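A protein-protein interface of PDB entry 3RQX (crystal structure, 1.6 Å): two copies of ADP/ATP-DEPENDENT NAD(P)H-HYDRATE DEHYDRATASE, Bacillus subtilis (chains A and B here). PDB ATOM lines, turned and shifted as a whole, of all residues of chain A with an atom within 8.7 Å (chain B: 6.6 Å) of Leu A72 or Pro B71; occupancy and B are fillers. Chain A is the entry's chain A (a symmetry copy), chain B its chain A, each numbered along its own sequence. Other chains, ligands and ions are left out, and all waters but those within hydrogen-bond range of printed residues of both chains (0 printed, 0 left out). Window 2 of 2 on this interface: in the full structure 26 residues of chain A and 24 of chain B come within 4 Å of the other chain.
The guanidinium group (NH2) of Arg B84 is in hydrogen-bond range of the backbone carbonyl oxygen (O) of Asp A40, 3.1 Å away.
The side-chain amide nitrogen (ND2) of Asn A68 sits at hydrogen-bond distance from the side-chain carboxylate (OD2) of Asp A40 (3.3 Å).
The side-chain carboxylate of Glu B67 lies within salt-bridge range of the guanidinium group of Arg B84.
CG of Pro A43 touches CG2 of Val B74, at 3.6 Å.
Leu A47 touches Pro B75 (CD2 to O, 3.9 Å).
CD2 of Leu A72 touches CB of Pro B71, at 3.5 Å.
CB of Val B74 touches CD1 of Leu A72, at 3.9 Å.
O of Leu A72 touches CB of Pro B75, 3.8 Å away.
CG2 of Val A76 touches O of Pro B75 (3.5 Å).
Of the printed residues of chain B, Asp A40 touches Arg B84.
Ile A63 touches none of the printed residues of chain B.
Of chain B, only Pro B71 (3.5 Å), Val B74 (3.9 Å) and Pro B75 (3.8 Å) come within 4 Å of Leu A72.
Printed residues of chain B within 4 Å of Val A76: Pro B75.
Pro B71 touches just one residue of chain A: Leu A72.
Of the printed residues of chain A, Pro B75 touches Leu A47 (3.9 Å), Leu A72 (3.8 Å) and Val A76 (3.5 Å).
The nearest residue of chain A that does not touch Pro B71 is Asn A68 (6.0 Å).
The nearest printed residue of chain A that does not touch Arg B84 is Asp A41 (4.1 Å).
Printed residues of chain B that touch a printed residue of chain A: Pro B71, Val B74, Pro B75 and Arg B84.
Of the 26 printed residues of chain A, 5 touch a printed residue of chain B.
Hydrophobic or aromatic side chains of chain A within 4 Å of the printed part of chain B: Pro A43, Leu A47, Leu A72 and Val A76.
Among the printed residues, no Asp or Glu carboxylate lies within 4 Å of a Lys or Arg side-chain nitrogen of the other chain.
Leu A72 touches Pro B71, but with the chains exchanged Pro A71 does not touch Leu B72 (8.6 Å).
Leu A72 touches Val B74, but with the chains exchanged Val A74 does not touch Leu B72 (11.9 Å).
Leu A72 touches Pro B75, but with the chains exchanged Pro A75 does not touch Leu B72 (9.4 Å).
Val A76 touches Pro B75, but with the chains exchanged Pro A75 does not touch Val B76 (8.4 Å).
Positions printed for both chains: 66, 67, 68, 69, 70, 71, 72, 73, 74, 75, 76 and 82.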
ATOM      1  N   SER A  39     -24.622 -29.692  15.795  1.00  0.00           N
ATOM      2  CA  SER A  39     -24.708 -30.887  14.913  1.00  0.00           C
ATOM      3  C   SER A  39     -26.133 -31.019  14.531  1.00  0.00           C
ATOM      4  O   SER A  39     -27.035 -30.330  15.098  1.00  0.00           O
ATOM      5  CB  SER A  39     -24.208 -32.099  15.645  1.00  0.00           C
ATOM      6  OG  SER A  39     -24.965 -32.342  16.815  1.00  0.00           O
ATOM      7  N   ASP A  40     -26.387 -31.919  13.573  1.00  0.00           N
ATOM      8  CA  ASP A  40     -27.720 -31.975  13.046  1.00  0.00           C
ATOM      9  C   ASP A  40     -28.675 -32.306  14.161  1.00  0.00           C
ATOM     10  O   ASP A  40     -29.834 -31.872  14.209  1.00  0.00           O
ATOM     11  CB  ASP A  40     -27.776 -33.020  11.904  1.00  0.00           C
ATOM     12  CG  ASP A  40     -27.085 -32.559  10.640  1.00  0.00           C
ATOM     13  OD1 ASP A  40     -26.575 -31.471  10.553  1.00  0.00           O
ATOM     14  OD2 ASP A  40     -27.143 -33.326   9.647  1.00  0.00           O
ATOM     15  N   ASP A  41     -28.207 -33.144  15.080  1.00  0.00           N
ATOM     16  CA  ASP A  41     -29.042 -33.555  16.165  1.00  0.00           C
ATOM     17  C   ASP A  41     -29.211 -32.492  17.308  1.00  0.00           C
ATOM     18  O   ASP A  41     -30.212 -32.440  18.025  1.00  0.00           O
ATOM     19  CB  ASP A  41     -28.421 -34.858  16.772  1.00  0.00           C
ATOM     20  CG  ASP A  41     -28.620 -36.137  15.930  1.00  0.00           C
ATOM     21  OD1 ASP A  41     -29.284 -36.153  14.896  1.00  0.00           O
ATOM     22  OD2 ASP A  41     -28.050 -37.166  16.368  1.00  0.00           O
ATOM     23  N   MET A  42     -28.224 -31.620  17.484  1.00  0.00           N
ATOM     24  CA  MET A  42     -28.245 -30.574  18.519  1.00  0.00           C
ATOM     25  C   MET A  42     -27.792 -29.234  17.887  1.00  0.00           C
ATOM     26  O   MET A  42     -26.695 -28.702  18.161  1.00  0.00           O
ATOM     27  CB  MET A  42     -27.272 -30.927  19.668  1.00  0.00           C
ATOM     28  CG  MET A  42     -27.738 -32.126  20.443  1.00  0.00           C
ATOM     29  SD  MET A  42     -26.368 -32.721  21.560  1.00  0.00           S
ATOM     30  CE  MET A  42     -25.254 -33.582  20.444  1.00  0.00           C
ATOM     31  N   PRO A  43     -28.657 -28.621  17.059  1.00  0.00           N
ATOM     32  CA  PRO A  43     -28.253 -27.481  16.295  1.00  0.00           C
ATOM     33  C   PRO A  43     -28.231 -26.181  17.112  1.00  0.00           C
ATOM     34  O   PRO A  43     -27.416 -25.292  16.852  1.00  0.00           O
ATOM     35  CB  PRO A  43     -29.314 -27.386  15.196  1.00  0.00           C
ATOM     36  CG  PRO A  43     -30.512 -28.044  15.799  1.00  0.00           C
ATOM     37  CD  PRO A  43     -29.931 -29.197  16.591  1.00  0.00           C
ATOM     38  N   GLY A  44     -29.201 -26.027  18.063  1.00  0.00           N
ATOM     39  CA  GLY A  44     -29.391 -24.755  18.712  1.00  0.00           C
ATOM     40  C   GLY A  44     -28.219 -24.237  19.479  1.00  0.00           C
ATOM     41  O   GLY A  44     -27.994 -23.019  19.535  1.00  0.00           O
ATOM     42  N   ALA A  46     -25.177 -24.090  18.655  1.00  0.00           N
ATOM     43  CA  ALA A  46     -24.298 -23.284  17.813  1.00  0.00           C
ATOM     44  C   ALA A  46     -24.831 -21.859  17.669  1.00  0.00           C
ATOM     45  O   ALA A  46     -24.080 -20.898  17.621  1.00  0.00           O
ATOM     46  CB  ALA A  46     -24.122 -23.942  16.429  1.00  0.00           C
ATOM     47  N   LEU A  47     -26.162 -21.694  17.560  1.00  0.00           N
ATOM     48  CA  LEU A  47     -26.734 -20.373  17.483  1.00  0.00           C
ATOM     49  C   LEU A  47     -26.510 -19.639  18.839  1.00  0.00           C
ATOM     50  O   LEU A  47     -26.151 -18.437  18.870  1.00  0.00           O
ATOM     51  CB  LEU A  47     -28.211 -20.394  17.115  1.00  0.00           C
ATOM     52  CG  LEU A  47     -28.896 -19.029  17.055  1.00  0.00           C
ATOM     53  CD1 LEU A  47     -28.085 -17.974  16.236  1.00  0.00           C
ATOM     54  CD2 LEU A  47     -30.335 -19.240  16.483  1.00  0.00           C
ATOM     55  N   LEU A  48     -26.761 -20.363  19.927  1.00  0.00           N
ATOM     56  CA  LEU A  48     -26.627 -19.750  21.264  1.00  0.00           C
ATOM     57  C   LEU A  48     -25.172 -19.297  21.501  1.00  0.00           C
ATOM     58  O   LEU A  48     -24.926 -18.157  21.927  1.00  0.00           O
ATOM     59  CB  LEU A  48     -27.076 -20.697  22.345  1.00  0.00           C
ATOM     60  CG  LEU A  48     -28.575 -20.970  22.384  1.00  0.00           C
ATOM     61  CD1 LEU A  48     -28.857 -22.124  23.286  1.00  0.00           C
ATOM     62  CD2 LEU A  48     -29.312 -19.641  22.792  1.00  0.00           C
ATOM     63  N   LEU A  51     -24.152 -16.302  19.034  1.00  0.00           N
ATOM     64  CA  LEU A  51     -24.672 -15.020  19.482  1.00  0.00           C
ATOM     65  C   LEU A  51     -23.850 -14.534  20.685  1.00  0.00           C
ATOM     66  O   LEU A  51     -23.457 -13.376  20.756  1.00  0.00           O
ATOM     67  CB  LEU A  51     -26.123 -15.176  19.870  1.00  0.00           C
ATOM     68  CG  LEU A  51     -27.100 -15.204  18.763  1.00  0.00           C
ATOM     69  CD1 LEU A  51     -28.445 -15.820  19.273  1.00  0.00           C
ATOM     70  CD2 LEU A  51     -27.380 -13.805  18.113  1.00  0.00           C
ATOM     71  N   ILE A  63     -17.827 -19.965  12.365  1.00  0.00           N
ATOM     72  CA  ILE A  63     -18.578 -21.074  12.959  1.00  0.00           C
ATOM     73  C   ILE A  63     -18.356 -22.317  12.100  1.00  0.00           C
ATOM     74  O   ILE A  63     -18.758 -22.352  10.959  1.00  0.00           O
ATOM     75  CB  ILE A  63     -20.050 -20.785  13.100  1.00  0.00           C
ATOM     76  CG1 ILE A  63     -20.272 -19.480  13.880  1.00  0.00           C
ATOM     77  CG2 ILE A  63     -20.715 -21.982  13.819  1.00  0.00           C
ATOM     78  CD1 ILE A  63     -21.752 -19.133  14.085  1.00  0.00           C
ATOM     79  N   THR A  65     -19.656 -25.489  11.901  1.00  0.00           N
ATOM     80  CA  THR A  65     -20.803 -26.274  12.305  1.00  0.00           C
ATOM     81  C   THR A  65     -21.168 -27.187  11.133  1.00  0.00           C
ATOM     82  O   THR A  65     -20.684 -27.049  10.000  1.00  0.00           O
ATOM     83  CB  THR A  65     -21.963 -25.417  12.695  1.00  0.00           C
ATOM     84  OG1 THR A  65     -23.010 -26.213  13.261  1.00  0.00           O
ATOM     85  CG2 THR A  65     -22.566 -24.654  11.499  1.00  0.00           C
ATOM     86  N   SER A  66     -22.053 -28.167  11.413  1.00  0.00           N
ATOM     87  CA  SER A  66     -22.545 -29.038  10.383  1.00  0.00           C
ATOM     88  C   SER A  66     -23.236 -28.277   9.292  1.00  0.00           C
ATOM     89  O   SER A  66     -23.896 -27.258   9.548  1.00  0.00           O
ATOM     90  CB  SER A  66     -23.515 -30.050  11.048  1.00  0.00           C
ATOM     91  OG  SER A  66     -22.757 -30.925  11.922  1.00  0.00           O
ATOM     92  N   GLU A  67     -23.106 -28.713   8.044  1.00  0.00           N
ATOM     93  CA  GLU A  67     -23.659 -28.017   6.936  1.00  0.00           C
ATOM     94  C   GLU A  67     -25.143 -27.661   7.094  1.00  0.00           C
ATOM     95  O   GLU A  67     -25.537 -26.565   6.759  1.00  0.00           O
ATOM     96  CB  GLU A  67     -23.447 -28.865   5.649  1.00  0.00           C
ATOM     97  CG  GLU A  67     -24.263 -28.570   4.471  1.00  0.00           C
ATOM     98  CD  GLU A  67     -23.660 -29.248   3.219  1.00  0.00           C
ATOM     99  OE1 GLU A  67     -23.495 -30.491   3.236  1.00  0.00           O
ATOM    100  OE2 GLU A  67     -23.370 -28.541   2.240  1.00  0.00           O
ATOM    101  N   ASN A  68     -25.940 -28.591   7.616  1.00  0.00           N
ATOM    102  CA  ASN A  68     -27.372 -28.365   7.760  1.00  0.00           C
ATOM    103  C   ASN A  68     -27.746 -27.397   8.865  1.00  0.00           C
ATOM    104  O   ASN A  68     -28.890 -26.998   8.963  1.00  0.00           O
ATOM    105  CB  ASN A  68     -28.091 -29.686   7.922  1.00  0.00           C
ATOM    106  CG  ASN A  68     -27.991 -30.543   6.679  1.00  0.00           C
ATOM    107  OD1 ASN A  68     -27.856 -30.023   5.563  1.00  0.00           O
ATOM    108  ND2 ASN A  68     -28.114 -31.849   6.850  1.00  0.00           N
ATOM    109  N   VAL A  69     -26.793 -27.079   9.717  1.00  0.00           N
ATOM    110  CA  VAL A  69     -27.003 -26.132  10.807  1.00  0.00           C
ATOM    111  C   VAL A  69     -26.803 -24.713  10.336  1.00  0.00           C
ATOM    112  O   VAL A  69     -27.403 -23.765  10.861  1.00  0.00           O
ATOM    113  CB  VAL A  69     -26.159 -26.469  12.008  1.00  0.00           C
ATOM    114  CG1 VAL A  69     -26.376 -25.464  13.217  1.00  0.00           C
ATOM    115  CG2 VAL A  69     -26.454 -27.890  12.504  1.00  0.00           C
ATOM    116  N   ILE A  70     -25.890 -24.486   9.392  1.00  0.00           N
ATOM    117  CA  ILE A  70     -25.594 -23.127   8.880  1.00  0.00           C
ATOM    118  C   ILE A  70     -26.859 -22.319   8.554  1.00  0.00           C
ATOM    119  O   ILE A  70     -26.958 -21.196   9.015  1.00  0.00           O
ATOM    120  CB  ILE A  70     -24.682 -23.206   7.643  1.00  0.00           C
ATOM    121  CG1 ILE A  70     -23.319 -23.733   8.083  1.00  0.00           C
ATOM    122  CG2 ILE A  70     -24.471 -21.835   6.987  1.00  0.00           C
ATOM    123  CD1 ILE A  70     -22.333 -23.996   6.878  1.00  0.00           C
ATOM    124  N   PRO A  71     -27.813 -22.862   7.799  1.00  0.00           N
ATOM    125  CA  PRO A  71     -29.014 -22.055   7.430  1.00  0.00           C
ATOM    126  C   PRO A  71     -29.863 -21.630   8.622  1.00  0.00           C
ATOM    127  O   PRO A  71     -30.683 -20.727   8.503  1.00  0.00           O
ATOM    128  CB  PRO A  71     -29.771 -22.923   6.450  1.00  0.00           C
ATOM    129  CG  PRO A  71     -29.266 -24.270   6.706  1.00  0.00           C
ATOM    130  CD  PRO A  71     -27.858 -24.175   7.105  1.00  0.00           C
ATOM    131  N   LEU A  72     -29.689 -22.318   9.749  1.00  0.00           N
ATOM    132  CA  LEU A  72     -30.480 -22.044  10.949  1.00  0.00           C
ATOM    133  C   LEU A  72     -29.880 -20.884  11.713  1.00  0.00           C
ATOM    134  O   LEU A  72     -30.542 -20.262  12.571  1.00  0.00           O
ATOM    135  CB  LEU A  72     -30.590 -23.312  11.817  1.00  0.00           C
ATOM    136  CG  LEU A  72     -31.005 -24.574  11.088  1.00  0.00           C
ATOM    137  CD1 LEU A  72     -31.127 -25.759  12.068  1.00  0.00           C
ATOM    138  CD2 LEU A  72     -32.184 -24.351  10.204  1.00  0.00           C
ATOM    139  N   ILE A  73     -28.602 -20.577  11.483  1.00  0.00           N
ATOM    140  CA  ILE A  73     -27.927 -19.500  12.169  1.00  0.00           C
ATOM    141  C   ILE A  73     -28.024 -18.183  11.426  1.00  0.00           C
ATOM    142  O   ILE A  73     -28.252 -17.133  12.024  1.00  0.00           O
ATOM    143  CB  ILE A  73     -26.440 -19.875  12.404  1.00  0.00           C
ATOM    144  CG1 ILE A  73     -26.326 -21.148  13.276  1.00  0.00           C
ATOM    145  CG2 ILE A  73     -25.675 -18.700  13.042  1.00  0.00           C
ATOM    146  CD1 ILE A  73     -24.852 -21.672  13.291  1.00  0.00           C
ATOM    147  N   VAL A  74     -27.867 -18.232  10.127  1.00  0.00           N
ATOM    148  CA  VAL A  74     -27.726 -17.041   9.290  1.00  0.00           C
ATOM    149  C   VAL A  74     -28.796 -15.961   9.504  1.00  0.00           C
ATOM    150  O   VAL A  74     -28.473 -14.817   9.659  1.00  0.00           O
ATOM    151  CB  VAL A  74     -27.613 -17.423   7.806  1.00  0.00           C
ATOM    152  CG1 VAL A  74     -27.629 -16.146   6.905  1.00  0.00           C
ATOM    153  CG2 VAL A  74     -26.357 -18.288   7.520  1.00  0.00           C
ATOM    154  N   PRO A  75     -30.085 -16.312   9.530  1.00  0.00           N
ATOM    155  CA  PRO A  75     -31.086 -15.242   9.658  1.00  0.00           C
ATOM    156  C   PRO A  75     -31.022 -14.529  10.968  1.00  0.00           C
ATOM    157  O   PRO A  75     -31.472 -13.379  11.037  1.00  0.00           O
ATOM    158  CB  PRO A  75     -32.446 -15.986   9.504  1.00  0.00           C
ATOM    159  CG  PRO A  75     -32.109 -17.362   9.044  1.00  0.00           C
ATOM    160  CD  PRO A  75     -30.674 -17.647   9.291  1.00  0.00           C
ATOM    161  N   VAL A  76     -30.527 -15.191  12.014  1.00  0.00           N
ATOM    162  CA  VAL A  76     -30.450 -14.606  13.357  1.00  0.00           C
ATOM    163  C   VAL A  76     -29.121 -13.891  13.577  1.00  0.00           C
ATOM    164  O   VAL A  76     -29.084 -12.853  14.278  1.00  0.00           O
ATOM    165  CB  VAL A  76     -30.682 -15.637  14.417  1.00  0.00           C
ATOM    166  CG1 VAL A  76     -30.650 -15.067  15.818  1.00  0.00           C
ATOM    167  CG2 VAL A  76     -32.069 -16.352  14.132  1.00  0.00           C
ATOM    168  N   LEU A  77     -28.054 -14.424  12.982  1.00  0.00           N
ATOM    169  CA  LEU A  77     -26.688 -13.947  13.216  1.00  0.00           C
ATOM    170  C   LEU A  77     -26.013 -13.850  11.856  1.00  0.00           C
ATOM    171  O   LEU A  77     -25.094 -14.641  11.537  1.00  0.00           O
ATOM    172  CB  LEU A  77     -25.962 -14.928  14.137  1.00  0.00           C
ATOM    173  CG  LEU A  77     -24.577 -14.436  14.601  1.00  0.00           C
ATOM    174  CD1 LEU A  77     -24.591 -13.156  15.441  1.00  0.00           C
ATOM    175  CD2 LEU A  77     -23.904 -15.592  15.364  1.00  0.00           C
ATOM    176  N   PRO A  78     -26.449 -12.891  11.025  1.00  0.00           N
ATOM    177  CA  PRO A  78     -25.883 -12.816   9.656  1.00  0.00           C
ATOM    178  C   PRO A  78     -24.425 -12.307   9.646  1.00  0.00           C
ATOM    179  O   PRO A  78     -23.791 -12.343   8.580  1.00  0.00           O
ATOM    180  CB  PRO A  78     -26.835 -11.860   8.924  1.00  0.00           C
ATOM    181  CG  PRO A  78     -27.383 -11.014  10.076  1.00  0.00           C
ATOM    182  CD  PRO A  78     -27.602 -11.991  11.202  1.00  0.00           C
ATOM    183  N   TYR A  82     -18.554 -18.962   8.089  1.00  0.00           N
ATOM    184  CA  TYR A  82     -18.637 -20.402   8.298  1.00  0.00           C
ATOM    185  C   TYR A  82     -17.424 -21.170   7.783  1.00  0.00           C
ATOM    186  O   TYR A  82     -16.860 -20.818   6.765  1.00  0.00           O
ATOM    187  CB  TYR A  82     -19.918 -21.002   7.696  1.00  0.00           C
ATOM    188  CG  TYR A  82     -21.117 -20.346   8.271  1.00  0.00           C
ATOM    189  CD1 TYR A  82     -21.636 -20.761   9.464  1.00  0.00           C
ATOM    190  CD2 TYR A  82     -21.663 -19.235   7.652  1.00  0.00           C
ATOM    191  CE1 TYR A  82     -22.680 -20.101  10.073  1.00  0.00           C
ATOM    192  CE2 TYR A  82     -22.687 -18.529   8.264  1.00  0.00           C
ATOM    193  CZ  TYR A  82     -23.194 -18.965   9.480  1.00  0.00           C
ATOM    194  OH  TYR A  82     -24.209 -18.277  10.129  1.00  0.00           O
ATOM    195  N   SER B  66     -41.555 -33.817  13.341  1.00  0.00           N
ATOM    196  CA  SER B  66     -41.106 -34.289  12.062  1.00  0.00           C
ATOM    197  C   SER B  66     -39.799 -33.670  11.666  1.00  0.00           C
ATOM    198  O   SER B  66     -39.533 -32.497  11.973  1.00  0.00           O
ATOM    199  CB  SER B  66     -42.209 -33.956  11.025  1.00  0.00           C
ATOM    200  OG  SER B  66     -43.382 -34.761  11.309  1.00  0.00           O
ATOM    201  N   GLU B  67     -38.928 -34.416  10.997  1.00  0.00           N
ATOM    202  CA  GLU B  67     -37.636 -33.944  10.645  1.00  0.00           C
ATOM    203  C   GLU B  67     -37.635 -32.580   9.941  1.00  0.00           C
ATOM    204  O   GLU B  67     -36.811 -31.746  10.247  1.00  0.00           O
ATOM    205  CB  GLU B  67     -36.934 -35.007   9.753  1.00  0.00           C
ATOM    206  CG  GLU B  67     -35.786 -34.597   8.943  1.00  0.00           C
ATOM    207  CD  GLU B  67     -35.019 -35.838   8.433  1.00  0.00           C
ATOM    208  OE1 GLU B  67     -35.646 -36.689   7.758  1.00  0.00           O
ATOM    209  OE2 GLU B  67     -33.811 -35.944   8.702  1.00  0.00           O
ATOM    210  N   ASN B  68     -38.570 -32.372   9.017  1.00  0.00           N
ATOM    211  CA  ASN B  68     -38.620 -31.129   8.258  1.00  0.00           C
ATOM    212  C   ASN B  68     -39.109 -29.932   9.050  1.00  0.00           C
ATOM    213  O   ASN B  68     -39.027 -28.815   8.578  1.00  0.00           O
ATOM    214  CB  ASN B  68     -39.434 -31.323   6.998  1.00  0.00           C
ATOM    215  CG  ASN B  68     -38.777 -32.294   6.042  1.00  0.00           C
ATOM    216  OD1 ASN B  68     -37.547 -32.439   6.035  1.00  0.00           O
ATOM    217  ND2 ASN B  68     -39.576 -32.919   5.193  1.00  0.00           N
ATOM    218  N   VAL B  69     -39.666 -30.185  10.216  1.00  0.00           N
ATOM    219  CA  VAL B  69     -40.149 -29.126  11.098  1.00  0.00           C
ATOM    220  C   VAL B  69     -39.031 -28.586  11.955  1.00  0.00           C
ATOM    221  O   VAL B  69     -39.033 -27.416  12.359  1.00  0.00           O
ATOM    222  CB  VAL B  69     -41.337 -29.575  11.908  1.00  0.00           C
ATOM    223  CG1 VAL B  69     -41.894 -28.441  12.868  1.00  0.00           C
ATOM    224  CG2 VAL B  69     -42.479 -30.038  10.995  1.00  0.00           C
ATOM    225  N   ILE B  70     -38.076 -29.428  12.347  1.00  0.00           N
ATOM    226  CA  ILE B  70     -36.950 -29.007  13.214  1.00  0.00           C
ATOM    227  C   ILE B  70     -36.299 -27.693  12.759  1.00  0.00           C
ATOM    228  O   ILE B  70     -36.146 -26.811  13.585  1.00  0.00           O
ATOM    229  CB  ILE B  70     -35.892 -30.121  13.299  1.00  0.00           C
ATOM    230  CG1 ILE B  70     -36.500 -31.307  14.043  1.00  0.00           C
ATOM    231  CG2 ILE B  70     -34.637 -29.675  14.062  1.00  0.00           C
ATOM    232  CD1 ILE B  70     -35.558 -32.575  14.071  1.00  0.00           C
ATOM    233  N   PRO B  71     -35.938 -27.542  11.486  1.00  0.00           N
ATOM    234  CA  PRO B  71     -35.249 -26.288  11.056  1.00  0.00           C
ATOM    235  C   PRO B  71     -36.095 -25.031  11.217  1.00  0.00           C
ATOM    236  O   PRO B  71     -35.565 -23.926  11.198  1.00  0.00           O
ATOM    237  CB  PRO B  71     -34.847 -26.546   9.621  1.00  0.00           C
ATOM    238  CG  PRO B  71     -35.725 -27.636   9.198  1.00  0.00           C
ATOM    239  CD  PRO B  71     -35.987 -28.501  10.353  1.00  0.00           C
ATOM    240  N   LEU B  72     -37.410 -25.212  11.328  1.00  0.00           N
ATOM    241  CA  LEU B  72     -38.336 -24.085  11.434  1.00  0.00           C
ATOM    242  C   LEU B  72     -38.409 -23.605  12.867  1.00  0.00           C
ATOM    243  O   LEU B  72     -38.863 -22.477  13.151  1.00  0.00           O
ATOM    244  CB  LEU B  72     -39.721 -24.478  10.886  1.00  0.00           C
ATOM    245  CG  LEU B  72     -39.724 -25.144   9.524  1.00  0.00           C
ATOM    246  CD1 LEU B  72     -41.167 -25.444   9.063  1.00  0.00           C
ATOM    247  CD2 LEU B  72     -38.878 -24.413   8.539  1.00  0.00           C
ATOM    248  N   ILE B  73     -38.024 -24.447  13.829  1.00  0.00           N
ATOM    249  CA  ILE B  73     -38.068 -24.098  15.229  1.00  0.00           C
ATOM    250  C   ILE B  73     -36.773 -23.482  15.719  1.00  0.00           C
ATOM    251  O   ILE B  73     -36.778 -22.505  16.465  1.00  0.00           O
ATOM    252  CB  ILE B  73     -38.419 -25.350  16.074  1.00  0.00           C
ATOM    253  CG1 ILE B  73     -39.804 -25.912  15.674  1.00  0.00           C
ATOM    254  CG2 ILE B  73     -38.371 -25.025  17.579  1.00  0.00           C
ATOM    255  CD1 ILE B  73     -40.038 -27.313  16.331  1.00  0.00           C
ATOM    256  N   VAL B  74     -35.665 -24.036  15.294  1.00  0.00           N
ATOM    257  CA  VAL B  74     -34.345 -23.702  15.826  1.00  0.00           C
ATOM    258  C   VAL B  74     -34.023 -22.202  15.881  1.00  0.00           C
ATOM    259  O   VAL B  74     -33.582 -21.718  16.886  1.00  0.00           O
ATOM    260  CB  VAL B  74     -33.243 -24.478  15.087  1.00  0.00           C
ATOM    261  CG1 VAL B  74     -31.828 -23.997  15.545  1.00  0.00           C
ATOM    262  CG2 VAL B  74     -33.391 -26.012  15.266  1.00  0.00           C
ATOM    263  N   PRO B  75     -34.253 -21.442  14.806  1.00  0.00           N
ATOM    264  CA  PRO B  75     -33.860 -20.027  14.868  1.00  0.00           C
ATOM    265  C   PRO B  75     -34.642 -19.241  15.867  1.00  0.00           C
ATOM    266  O   PRO B  75     -34.144 -18.206  16.327  1.00  0.00           O
ATOM    267  CB  PRO B  75     -34.130 -19.503  13.426  1.00  0.00           C
ATOM    268  CG  PRO B  75     -34.404 -20.710  12.597  1.00  0.00           C
ATOM    269  CD  PRO B  75     -34.723 -21.867  13.470  1.00  0.00           C
ATOM    270  N   VAL B  76     -35.865 -19.671  16.179  1.00  0.00           N
ATOM    271  CA  VAL B  76     -36.739 -18.960  17.118  1.00  0.00           C
ATOM    272  C   VAL B  76     -36.541 -19.457  18.546  1.00  0.00           C
ATOM    273  O   VAL B  76     -36.634 -18.651  19.501  1.00  0.00           O
ATOM    274  CB  VAL B  76     -38.176 -19.063  16.713  1.00  0.00           C
ATOM    275  CG1 VAL B  76     -39.110 -18.309  17.635  1.00  0.00           C
ATOM    276  CG2 VAL B  76     -38.319 -18.543  15.221  1.00  0.00           C
ATOM    277  N   TYR B  82     -34.015 -32.032  20.269  1.00  0.00           N
ATOM    278  CA  TYR B  82     -34.913 -32.754  19.376  1.00  0.00           C
ATOM    279  C   TYR B  82     -34.815 -34.272  19.500  1.00  0.00           C
ATOM    280  O   TYR B  82     -33.742 -34.804  19.711  1.00  0.00           O
ATOM    281  CB  TYR B  82     -34.721 -32.346  17.907  1.00  0.00           C
ATOM    282  CG  TYR B  82     -34.926 -30.886  17.744  1.00  0.00           C
ATOM    283  CD1 TYR B  82     -36.181 -30.370  17.591  1.00  0.00           C
ATOM    284  CD2 TYR B  82     -33.852 -30.020  17.850  1.00  0.00           C
ATOM    285  CE1 TYR B  82     -36.409 -29.013  17.548  1.00  0.00           C
ATOM    286  CE2 TYR B  82     -34.060 -28.649  17.851  1.00  0.00           C
ATOM    287  CZ  TYR B  82     -35.346 -28.147  17.701  1.00  0.00           C
ATOM    288  OH  TYR B  82     -35.594 -26.782  17.710  1.00  0.00           O
ATOM    289  N   ARG B  84     -35.714 -36.639  16.621  1.00  0.00           N
ATOM    290  CA  ARG B  84     -36.073 -36.568  15.220  1.00  0.00           C
ATOM    291  C   ARG B  84     -37.182 -37.539  14.887  1.00  0.00           C
ATOM    292  O   ARG B  84     -37.044 -38.709  15.152  1.00  0.00           O
ATOM    293  CB  ARG B  84     -34.820 -36.850  14.376  1.00  0.00           C
ATOM    294  CG  ARG B  84     -34.967 -36.676  12.881  1.00  0.00           C
ATOM    295  CD  ARG B  84     -33.535 -36.822  12.202  1.00  0.00           C
ATOM    296  NE  ARG B  84     -32.674 -35.712  12.631  1.00  0.00           N
ATOM    297  CZ  ARG B  84     -32.609 -34.517  12.045  1.00  0.00           C
ATOM    298  NH1 ARG B  84     -33.175 -34.297  10.865  1.00  0.00           N
ATOM    299  NH2 ARG B  84     -31.879 -33.551  12.588  1.00  0.00           N
